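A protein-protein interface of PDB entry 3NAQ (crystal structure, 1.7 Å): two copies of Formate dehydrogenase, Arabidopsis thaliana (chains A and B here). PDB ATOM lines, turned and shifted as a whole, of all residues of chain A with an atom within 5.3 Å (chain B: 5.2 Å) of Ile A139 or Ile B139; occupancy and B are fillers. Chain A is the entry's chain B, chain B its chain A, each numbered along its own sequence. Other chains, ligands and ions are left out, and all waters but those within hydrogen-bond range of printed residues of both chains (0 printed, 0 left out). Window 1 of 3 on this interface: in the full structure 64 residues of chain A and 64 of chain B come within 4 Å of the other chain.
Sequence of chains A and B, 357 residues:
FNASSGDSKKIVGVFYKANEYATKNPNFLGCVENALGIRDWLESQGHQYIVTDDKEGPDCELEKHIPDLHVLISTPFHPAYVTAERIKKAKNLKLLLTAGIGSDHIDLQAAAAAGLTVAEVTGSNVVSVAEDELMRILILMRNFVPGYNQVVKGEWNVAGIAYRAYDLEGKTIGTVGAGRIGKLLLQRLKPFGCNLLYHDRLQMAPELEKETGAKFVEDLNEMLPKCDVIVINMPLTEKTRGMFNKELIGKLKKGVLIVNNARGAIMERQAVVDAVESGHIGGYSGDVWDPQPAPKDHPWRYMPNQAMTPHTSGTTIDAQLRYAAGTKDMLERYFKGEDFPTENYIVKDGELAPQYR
The backbone carbonyl oxygen of Leu B138 lies close to the side-chain sulfur of Met A135 (3.6 Å).
The backbone carbonyl oxygen (O) of Leu A138 sits close to the side-chain sulfur (SD) of Met B135, at 3.6 Å.
Printed residues of chain B that touch a printed residue of chain A: Leu B134, Met B135, Leu B138, Ile B139, Phe B144, Val B145 and Ala B307.
Hydrophobic or aromatic side chains of chain B within 4 Å of the printed part of chain A: Leu B134, Met B135, Leu B138, Ile B139, Phe B144 and Val B145.
Among the printed residues, 14 pairs touch across the chains.
Among the printed residues, pairs that only touch across the chains: Phe A144 with Ala B307 (3.6 Å), Ile A139 with Phe B144 (3.6 Å), Ala A307 with Phe B144 (3.6 Å), Phe A144 with Ile B139 (3.7 Å), Phe A144 with Met B135 (3.8 Å), Met A135 with Phe B144 (3.8 Å), Met A135 with Ile B139 (3.9 Å), Ile A139 with Met B135 (3.9 Å), Phe A144 with Val B145 (3.95 Å), Ile A139 with Ile B139 (3.96 Å), Val A145 with Phe B144 (3.99 Å) and Leu A138 with Leu B134 (3.997 Å).
Met A135 touches Phe B144, and with the chains exchanged Phe A144 touches Met B135.
Leu A138 touches Leu B134, but with the chains exchanged Leu A134 does not touch Leu B138 (4.1 Å).
Ile A139 touches its own counterpart, Ile B139.
Phe A144 touches Val B145, and with the chains exchanged Val A145 touches Phe B144.
Of chain B, only Met B135 (3.9 Å), Ile B139 (3.96 Å) and Phe B144 (3.6 Å) come within 4 Å of Ile A139.
Printed residues of chain A within 4 Å of Ile B139: Met A135 (3.9 Å), Ile A139 (3.96 Å) and Phe A144 (3.7 Å).
Of the printed residues of chain A, Phe B144 touches Met A135, Ile A139, Val A145 and Ala A307.
Printed residues of chain B within 4 Å of Ala A307: Phe B144 (3.6 Å).
Leu A134 touches none of the printed residues of chain B.
Ile B137 touches none of the printed residues of chain A.
NH1 of Arg B136 sits at hydrogen-bond distance from O of Ala B307 (3.1 Å).
N of Phe B144 is in hydrogen-bond range of O of Ile B139 (3.1 Å).
The backbone carbonyl oxygen (O) of Ala A307 is in hydrogen-bond range of the guanidinium group (NH1) of Arg A136 (3.2 Å).
The backbone NH (N) of Phe A144 is in hydrogen-bond range of the backbone carbonyl oxygen (O) of Ile A139 (3.1 Å).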
ATOM      1  N   LEU A 134      -6.319  -6.500 -28.767  1.00  0.00           N
ATOM      2  CA  LEU A 134      -4.951  -6.159 -29.070  1.00  0.00           C
ATOM      3  C   LEU A 134      -4.325  -5.399 -27.893  1.00  0.00           C
ATOM      4  O   LEU A 134      -3.201  -5.702 -27.465  1.00  0.00           O
ATOM      5  CB  LEU A 134      -4.866  -5.363 -30.359  1.00  0.00           C
ATOM      6  CG  LEU A 134      -3.435  -5.499 -30.927  1.00  0.00           C
ATOM      7  CD1 LEU A 134      -3.423  -5.694 -32.382  1.00  0.00           C
ATOM      8  CD2 LEU A 134      -2.554  -4.336 -30.449  1.00  0.00           C
ATOM      9  N   MET A 135      -5.074  -4.450 -27.336  1.00  0.00           N
ATOM     10  CA  MET A 135      -4.646  -3.741 -26.144  1.00  0.00           C
ATOM     11  C   MET A 135      -4.221  -4.645 -25.030  1.00  0.00           C
ATOM     12  O   MET A 135      -3.164  -4.495 -24.405  1.00  0.00           O
ATOM     13  CB  MET A 135      -5.767  -2.821 -25.645  1.00  0.00           C
ATOM     14  CG  MET A 135      -5.381  -2.045 -24.479  1.00  0.00           C
ATOM     15  SD  MET A 135      -6.748  -1.050 -23.835  1.00  0.00           S
ATOM     16  CE  MET A 135      -7.795  -2.361 -23.075  1.00  0.00           C
ATOM     17  N   ARG A 136      -5.049  -5.622 -24.781  1.00  0.00           N
ATOM     18  CA  ARG A 136      -4.828  -6.575 -23.697  1.00  0.00           C
ATOM     19  C   ARG A 136      -3.648  -7.486 -23.976  1.00  0.00           C
ATOM     20  O   ARG A 136      -2.932  -7.809 -23.066  1.00  0.00           O
ATOM     21  CB  ARG A 136      -6.079  -7.369 -23.459  1.00  0.00           C
ATOM     22  CG  ARG A 136      -7.147  -6.494 -22.889  1.00  0.00           C
ATOM     23  CD  ARG A 136      -8.488  -7.259 -22.801  1.00  0.00           C
ATOM     24  NE  ARG A 136      -9.536  -6.301 -22.525  1.00  0.00           N
ATOM     25  CZ  ARG A 136      -9.900  -5.912 -21.300  1.00  0.00           C
ATOM     26  NH1 ARG A 136      -9.307  -6.408 -20.244  1.00  0.00           N
ATOM     27  NH2 ARG A 136     -10.849  -4.996 -21.147  1.00  0.00           N
ATOM     28  N   ILE A 137      -3.426  -7.837 -25.237  1.00  0.00           N
ATOM     29  CA  ILE A 137      -2.240  -8.616 -25.614  1.00  0.00           C
ATOM     30  C   ILE A 137      -1.000  -7.854 -25.178  1.00  0.00           C
ATOM     31  O   ILE A 137      -0.110  -8.391 -24.519  1.00  0.00           O
ATOM     32  CB  ILE A 137      -2.211  -8.955 -27.133  1.00  0.00           C
ATOM     33  CG1 ILE A 137      -3.350  -9.917 -27.508  1.00  0.00           C
ATOM     34  CG2 ILE A 137      -0.846  -9.565 -27.549  1.00  0.00           C
ATOM     35  CD1 ILE A 137      -3.516 -10.030 -29.042  1.00  0.00           C
ATOM     36  N   LEU A 138      -0.947  -6.585 -25.555  1.00  0.00           N
ATOM     37  CA  LEU A 138       0.197  -5.738 -25.185  1.00  0.00           C
ATOM     38  C   LEU A 138       0.309  -5.515 -23.677  1.00  0.00           C
ATOM     39  O   LEU A 138       1.394  -5.619 -23.116  1.00  0.00           O
ATOM     40  CB  LEU A 138       0.105  -4.401 -25.920  1.00  0.00           C
ATOM     41  CG  LEU A 138       0.392  -4.456 -27.401  1.00  0.00           C
ATOM     42  CD1 LEU A 138      -0.172  -3.246 -28.148  1.00  0.00           C
ATOM     43  CD2 LEU A 138       1.881  -4.627 -27.582  1.00  0.00           C
ATOM     44  N   ILE A 139      -0.816  -5.243 -23.002  1.00  0.00           N
ATOM     45  CA  ILE A 139      -0.812  -5.038 -21.553  1.00  0.00           C
ATOM     46  C   ILE A 139      -0.210  -6.247 -20.850  1.00  0.00           C
ATOM     47  O   ILE A 139       0.606  -6.104 -19.947  1.00  0.00           O
ATOM     48  CB  ILE A 139      -2.205  -4.750 -20.986  1.00  0.00           C
ATOM     49  CG1 ILE A 139      -2.679  -3.336 -21.296  1.00  0.00           C
ATOM     50  CG2 ILE A 139      -2.281  -5.061 -19.442  1.00  0.00           C
ATOM     51  CD1 ILE A 139      -4.240  -3.084 -21.077  1.00  0.00           C
ATOM     52  N   LEU A 140      -0.688  -7.441 -21.208  1.00  0.00           N
ATOM     53  CA  LEU A 140      -0.125  -8.628 -20.632  1.00  0.00           C
ATOM     54  C   LEU A 140       1.331  -8.881 -21.015  1.00  0.00           C
ATOM     55  O   LEU A 140       2.182  -9.113 -20.150  1.00  0.00           O
ATOM     56  CB  LEU A 140      -0.970  -9.825 -21.008  1.00  0.00           C
ATOM     57  CG  LEU A 140      -2.350  -9.826 -20.374  1.00  0.00           C
ATOM     58  CD1 LEU A 140      -3.043 -11.145 -20.874  1.00  0.00           C
ATOM     59  CD2 LEU A 140      -2.346  -9.729 -18.810  1.00  0.00           C
ATOM     60  N   MET A 141       1.602  -8.848 -22.304  1.00  0.00           N
ATOM     61  CA  MET A 141       2.960  -9.164 -22.810  1.00  0.00           C
ATOM     62  C   MET A 141       4.027  -8.233 -22.217  1.00  0.00           C
ATOM     63  O   MET A 141       5.086  -8.693 -21.766  1.00  0.00           O
ATOM     64  CB  MET A 141       3.003  -9.076 -24.330  1.00  0.00           C
ATOM     65  CG  MET A 141       4.293  -9.569 -24.920  1.00  0.00           C
ATOM     66  SD  MET A 141       4.719 -11.242 -24.541  1.00  0.00           S
ATOM     67  CE  MET A 141       3.434 -12.151 -25.507  1.00  0.00           C
ATOM     68  N   ARG A 142       3.720  -6.958 -22.236  1.00  0.00           N
ATOM     69  CA  ARG A 142       4.654  -5.902 -21.816  1.00  0.00           C
ATOM     70  C   ARG A 142       4.536  -5.591 -20.332  1.00  0.00           C
ATOM     71  O   ARG A 142       5.294  -4.798 -19.812  1.00  0.00           O
ATOM     72  CB  ARG A 142       4.448  -4.669 -22.685  1.00  0.00           C
ATOM     73  CG  ARG A 142       4.605  -4.912 -24.134  1.00  0.00           C
ATOM     74  CD  ARG A 142       4.709  -3.655 -24.997  1.00  0.00           C
ATOM     75  NE  ARG A 142       5.802  -2.868 -24.484  1.00  0.00           N
ATOM     76  CZ  ARG A 142       7.089  -3.106 -24.711  1.00  0.00           C
ATOM     77  NH1 ARG A 142       7.463  -3.983 -25.628  1.00  0.00           N
ATOM     78  NH2 ARG A 142       7.999  -2.411 -24.035  1.00  0.00           N
ATOM     79  N   ASN A 143       3.628  -6.275 -19.623  1.00  0.00           N
ATOM     80  CA  ASN A 143       3.537  -6.194 -18.165  1.00  0.00           C
ATOM     81  C   ASN A 143       3.241  -4.785 -17.632  1.00  0.00           C
ATOM     82  O   ASN A 143       3.894  -4.320 -16.697  1.00  0.00           O
ATOM     83  CB  ASN A 143       4.810  -6.764 -17.523  1.00  0.00           C
ATOM     84  CG  ASN A 143       4.568  -7.407 -16.199  1.00  0.00           C
ATOM     85  OD1 ASN A 143       3.513  -8.010 -15.987  1.00  0.00           O
ATOM     86  ND2 ASN A 143       5.552  -7.349 -15.337  1.00  0.00           N
ATOM     87  N   PHE A 144       2.256  -4.136 -18.245  1.00  0.00           N
ATOM     88  CA  PHE A 144       1.806  -2.810 -17.845  1.00  0.00           C
ATOM     89  C   PHE A 144       1.302  -2.744 -16.406  1.00  0.00           C
ATOM     90  O   PHE A 144       1.646  -1.832 -15.653  1.00  0.00           O
ATOM     91  CB  PHE A 144       0.694  -2.355 -18.759  1.00  0.00           C
ATOM     92  CG  PHE A 144       0.087  -1.075 -18.358  1.00  0.00           C
ATOM     93  CD1 PHE A 144       0.785   0.096 -18.494  1.00  0.00           C
ATOM     94  CD2 PHE A 144      -1.162  -1.039 -17.783  1.00  0.00           C
ATOM     95  CE1 PHE A 144       0.247   1.310 -18.102  1.00  0.00           C
ATOM     96  CE2 PHE A 144      -1.705   0.180 -17.358  1.00  0.00           C
ATOM     97  CZ  PHE A 144      -0.981   1.364 -17.522  1.00  0.00           C
ATOM     98  N   VAL A 145       0.475  -3.694 -16.040  1.00  0.00           N
ATOM     99  CA  VAL A 145      -0.257  -3.597 -14.793  1.00  0.00           C
ATOM    100  C   VAL A 145       0.632  -3.482 -13.546  1.00  0.00           C
ATOM    101  O   VAL A 145       0.430  -2.586 -12.763  1.00  0.00           O
ATOM    102  CB  VAL A 145      -1.327  -4.650 -14.647  1.00  0.00           C
ATOM    103  CG1 VAL A 145      -1.866  -4.646 -13.227  1.00  0.00           C
ATOM    104  CG2 VAL A 145      -2.501  -4.373 -15.616  1.00  0.00           C
ATOM    105  N   ALA A 307      -5.516  -8.721 -15.539  1.00  0.00           N
ATOM    106  CA  ALA A 307      -5.698  -7.422 -16.127  1.00  0.00           C
ATOM    107  C   ALA A 307      -7.123  -7.243 -16.625  1.00  0.00           C
ATOM    108  O   ALA A 307      -7.345  -6.860 -17.777  1.00  0.00           O
ATOM    109  CB  ALA A 307      -4.689  -7.215 -17.250  1.00  0.00           C
ATOM    110  N   LEU B 134       2.325   2.311 -28.579  1.00  0.00           N
ATOM    111  CA  LEU B 134       1.060   1.867 -29.141  1.00  0.00           C
ATOM    112  C   LEU B 134       0.124   1.327 -28.047  1.00  0.00           C
ATOM    113  O   LEU B 134      -1.052   1.693 -27.979  1.00  0.00           O
ATOM    114  CB  LEU B 134       1.277   0.847 -30.258  1.00  0.00           C
ATOM    115  CG  LEU B 134       0.019   0.822 -31.154  1.00  0.00           C
ATOM    116  CD1 LEU B 134       0.313   0.661 -32.572  1.00  0.00           C
ATOM    117  CD2 LEU B 134      -0.976  -0.238 -30.654  1.00  0.00           C
ATOM    118  N   MET B 135       0.687   0.546 -27.131  1.00  0.00           N
ATOM    119  CA  MET B 135      -0.032   0.076 -25.961  1.00  0.00           C
ATOM    120  C   MET B 135      -0.684   1.171 -25.182  1.00  0.00           C
ATOM    121  O   MET B 135      -1.870   1.106 -24.805  1.00  0.00           O
ATOM    122  CB  MET B 135       0.897  -0.718 -25.027  1.00  0.00           C
ATOM    123  CG  MET B 135       0.223  -1.201 -23.835  1.00  0.00           C
ATOM    124  SD  MET B 135       1.371  -2.043 -22.732  1.00  0.00           S
ATOM    125  CE  MET B 135       2.203  -0.600 -21.949  1.00  0.00           C
ATOM    126  N   ARG B 136       0.093   2.195 -24.921  1.00  0.00           N
ATOM    127  CA  ARG B 136      -0.385   3.331 -24.152  1.00  0.00           C
ATOM    128  C   ARG B 136      -1.438   4.128 -24.884  1.00  0.00           C
ATOM    129  O   ARG B 136      -2.366   4.628 -24.252  1.00  0.00           O
ATOM    130  CB  ARG B 136       0.782   4.227 -23.789  1.00  0.00           C
ATOM    131  CG  ARG B 136       1.658   3.557 -22.756  1.00  0.00           C
ATOM    132  CD  ARG B 136       2.978   4.331 -22.518  1.00  0.00           C
ATOM    133  NE  ARG B 136       3.898   3.459 -21.796  1.00  0.00           N
ATOM    134  CZ  ARG B 136       3.949   3.324 -20.474  1.00  0.00           C
ATOM    135  NH1 ARG B 136       3.132   3.980 -19.692  1.00  0.00           N
ATOM    136  NH2 ARG B 136       4.794   2.456 -19.948  1.00  0.00           N
ATOM    137  N   ILE B 137      -1.295   4.266 -26.204  1.00  0.00           N
ATOM    138  CA  ILE B 137      -2.360   4.906 -27.020  1.00  0.00           C
ATOM    139  C   ILE B 137      -3.699   4.224 -26.739  1.00  0.00           C
ATOM    140  O   ILE B 137      -4.705   4.860 -26.435  1.00  0.00           O
ATOM    141  CB  ILE B 137      -2.031   4.923 -28.539  1.00  0.00           C
ATOM    142  CG1 ILE B 137      -0.823   5.820 -28.803  1.00  0.00           C
ATOM    143  CG2 ILE B 137      -3.232   5.426 -29.376  1.00  0.00           C
ATOM    144  CD1 ILE B 137      -0.249   5.684 -30.210  1.00  0.00           C
ATOM    145  N   LEU B 138      -3.705   2.905 -26.848  1.00  0.00           N
ATOM    146  CA  LEU B 138      -4.929   2.138 -26.594  1.00  0.00           C
ATOM    147  C   LEU B 138      -5.388   2.216 -25.152  1.00  0.00           C
ATOM    148  O   LEU B 138      -6.587   2.387 -24.902  1.00  0.00           O
ATOM    149  CB  LEU B 138      -4.677   0.706 -26.971  1.00  0.00           C
ATOM    150  CG  LEU B 138      -4.596   0.433 -28.461  1.00  0.00           C
ATOM    151  CD1 LEU B 138      -3.949  -0.931 -28.728  1.00  0.00           C
ATOM    152  CD2 LEU B 138      -5.992   0.515 -29.051  1.00  0.00           C
ATOM    153  N   ILE B 139      -4.464   2.059 -24.201  1.00  0.00           N
ATOM    154  CA  ILE B 139      -4.805   2.180 -22.771  1.00  0.00           C
ATOM    155  C   ILE B 139      -5.556   3.489 -22.495  1.00  0.00           C
ATOM    156  O   ILE B 139      -6.597   3.515 -21.839  1.00  0.00           O
ATOM    157  CB  ILE B 139      -3.596   2.100 -21.849  1.00  0.00           C
ATOM    158  CG1 ILE B 139      -3.103   0.667 -21.782  1.00  0.00           C
ATOM    159  CG2 ILE B 139      -3.927   2.685 -20.421  1.00  0.00           C
ATOM    160  CD1 ILE B 139      -1.666   0.486 -21.176  1.00  0.00           C
ATOM    161  N   LEU B 140      -4.990   4.595 -22.957  1.00  0.00           N
ATOM    162  CA  LEU B 140      -5.642   5.866 -22.781  1.00  0.00           C
ATOM    163  C   LEU B 140      -6.951   6.002 -23.563  1.00  0.00           C
ATOM    164  O   LEU B 140      -7.989   6.372 -23.011  1.00  0.00           O
ATOM    165  CB  LEU B 140      -4.705   6.970 -23.176  1.00  0.00           C
ATOM    166  CG  LEU B 140      -3.501   7.186 -22.273  1.00  0.00           C
ATOM    167  CD1 LEU B 140      -2.664   8.348 -22.841  1.00  0.00           C
ATOM    168  CD2 LEU B 140      -3.914   7.443 -20.794  1.00  0.00           C
ATOM    169  N   MET B 141      -6.907   5.674 -24.837  1.00  0.00           N
ATOM    170  CA  MET B 141      -8.066   5.887 -25.716  1.00  0.00           C
ATOM    171  C   MET B 141      -9.264   5.060 -25.228  1.00  0.00           C
ATOM    172  O   MET B 141     -10.385   5.560 -25.152  1.00  0.00           O
ATOM    173  CB  MET B 141      -7.743   5.482 -27.144  1.00  0.00           C
ATOM    174  CG  MET B 141      -8.854   5.820 -28.119  1.00  0.00           C
ATOM    175  SD  MET B 141      -9.302   7.538 -28.197  1.00  0.00           S
ATOM    176  CE  MET B 141      -7.818   8.265 -28.991  1.00  0.00           C
ATOM    177  N   ARG B 142      -8.989   3.824 -24.919  1.00  0.00           N
ATOM    178  CA  ARG B 142     -10.022   2.847 -24.533  1.00  0.00           C
ATOM    179  C   ARG B 142     -10.302   2.844 -23.038  1.00  0.00           C
ATOM    180  O   ARG B 142     -11.176   2.120 -22.568  1.00  0.00           O
ATOM    181  CB  ARG B 142      -9.637   1.465 -25.050  1.00  0.00           C
ATOM    182  CG  ARG B 142      -9.412   1.394 -26.527  1.00  0.00           C
ATOM    183  CD  ARG B 142      -9.342  -0.029 -27.109  1.00  0.00           C
ATOM    184  NE  ARG B 142     -10.557  -0.727 -26.741  1.00  0.00           N
ATOM    185  CZ  ARG B 142     -11.747  -0.562 -27.323  1.00  0.00           C
ATOM    186  NH1 ARG B 142     -11.874   0.143 -28.427  1.00  0.00           N
ATOM    187  NH2 ARG B 142     -12.810  -1.129 -26.782  1.00  0.00           N
ATOM    188  N   ASN B 143      -9.570   3.665 -22.287  1.00  0.00           N
ATOM    189  CA  ASN B 143      -9.830   3.904 -20.865  1.00  0.00           C
ATOM    190  C   ASN B 143      -9.710   2.645 -20.005  1.00  0.00           C
ATOM    191  O   ASN B 143     -10.573   2.368 -19.188  1.00  0.00           O
ATOM    192  CB  ASN B 143     -11.224   4.521 -20.693  1.00  0.00           C
ATOM    193  CG  ASN B 143     -11.295   5.438 -19.522  1.00  0.00           C
ATOM    194  OD1 ASN B 143     -10.295   6.090 -19.186  1.00  0.00           O
ATOM    195  ND2 ASN B 143     -12.460   5.517 -18.899  1.00  0.00           N
ATOM    196  N   PHE B 144      -8.625   1.913 -20.219  1.00  0.00           N
ATOM    197  CA  PHE B 144      -8.326   0.703 -19.473  1.00  0.00           C
ATOM    198  C   PHE B 144      -8.192   0.948 -17.988  1.00  0.00           C
ATOM    199  O   PHE B 144      -8.735   0.192 -17.166  1.00  0.00           O
ATOM    200  CB  PHE B 144      -7.030   0.116 -19.987  1.00  0.00           C
ATOM    201  CG  PHE B 144      -6.567  -1.055 -19.215  1.00  0.00           C
ATOM    202  CD1 PHE B 144      -7.252  -2.248 -19.293  1.00  0.00           C
ATOM    203  CD2 PHE B 144      -5.485  -0.948 -18.356  1.00  0.00           C
ATOM    204  CE1 PHE B 144      -6.846  -3.352 -18.570  1.00  0.00           C
ATOM    205  CE2 PHE B 144      -5.096  -2.063 -17.578  1.00  0.00           C
ATOM    206  CZ  PHE B 144      -5.786  -3.253 -17.695  1.00  0.00           C
ATOM    207  N   VAL B 145      -7.431   1.965 -17.627  1.00  0.00           N
ATOM    208  CA  VAL B 145      -7.027   2.112 -16.229  1.00  0.00           C
ATOM    209  C   VAL B 145      -8.194   2.201 -15.233  1.00  0.00           C
ATOM    210  O   VAL B 145      -8.213   1.447 -14.281  1.00  0.00           O
ATOM    211  CB  VAL B 145      -5.993   3.195 -16.014  1.00  0.00           C
ATOM    212  CG1 VAL B 145      -5.863   3.523 -14.528  1.00  0.00           C
ATOM    213  CG2 VAL B 145      -4.601   2.745 -16.555  1.00  0.00           C
ATOM    214  N   ALA B 307      -1.587   7.097 -16.667  1.00  0.00           N
ATOM    215  CA  ALA B 307      -1.338   5.703 -16.918  1.00  0.00           C
ATOM    216  C   ALA B 307       0.157   5.457 -17.025  1.00  0.00           C
ATOM    217  O   ALA B 307       0.639   4.849 -18.005  1.00  0.00           O
ATOM    218  CB  ALA B 307      -2.070   5.281 -18.178  1.00  0.00           C
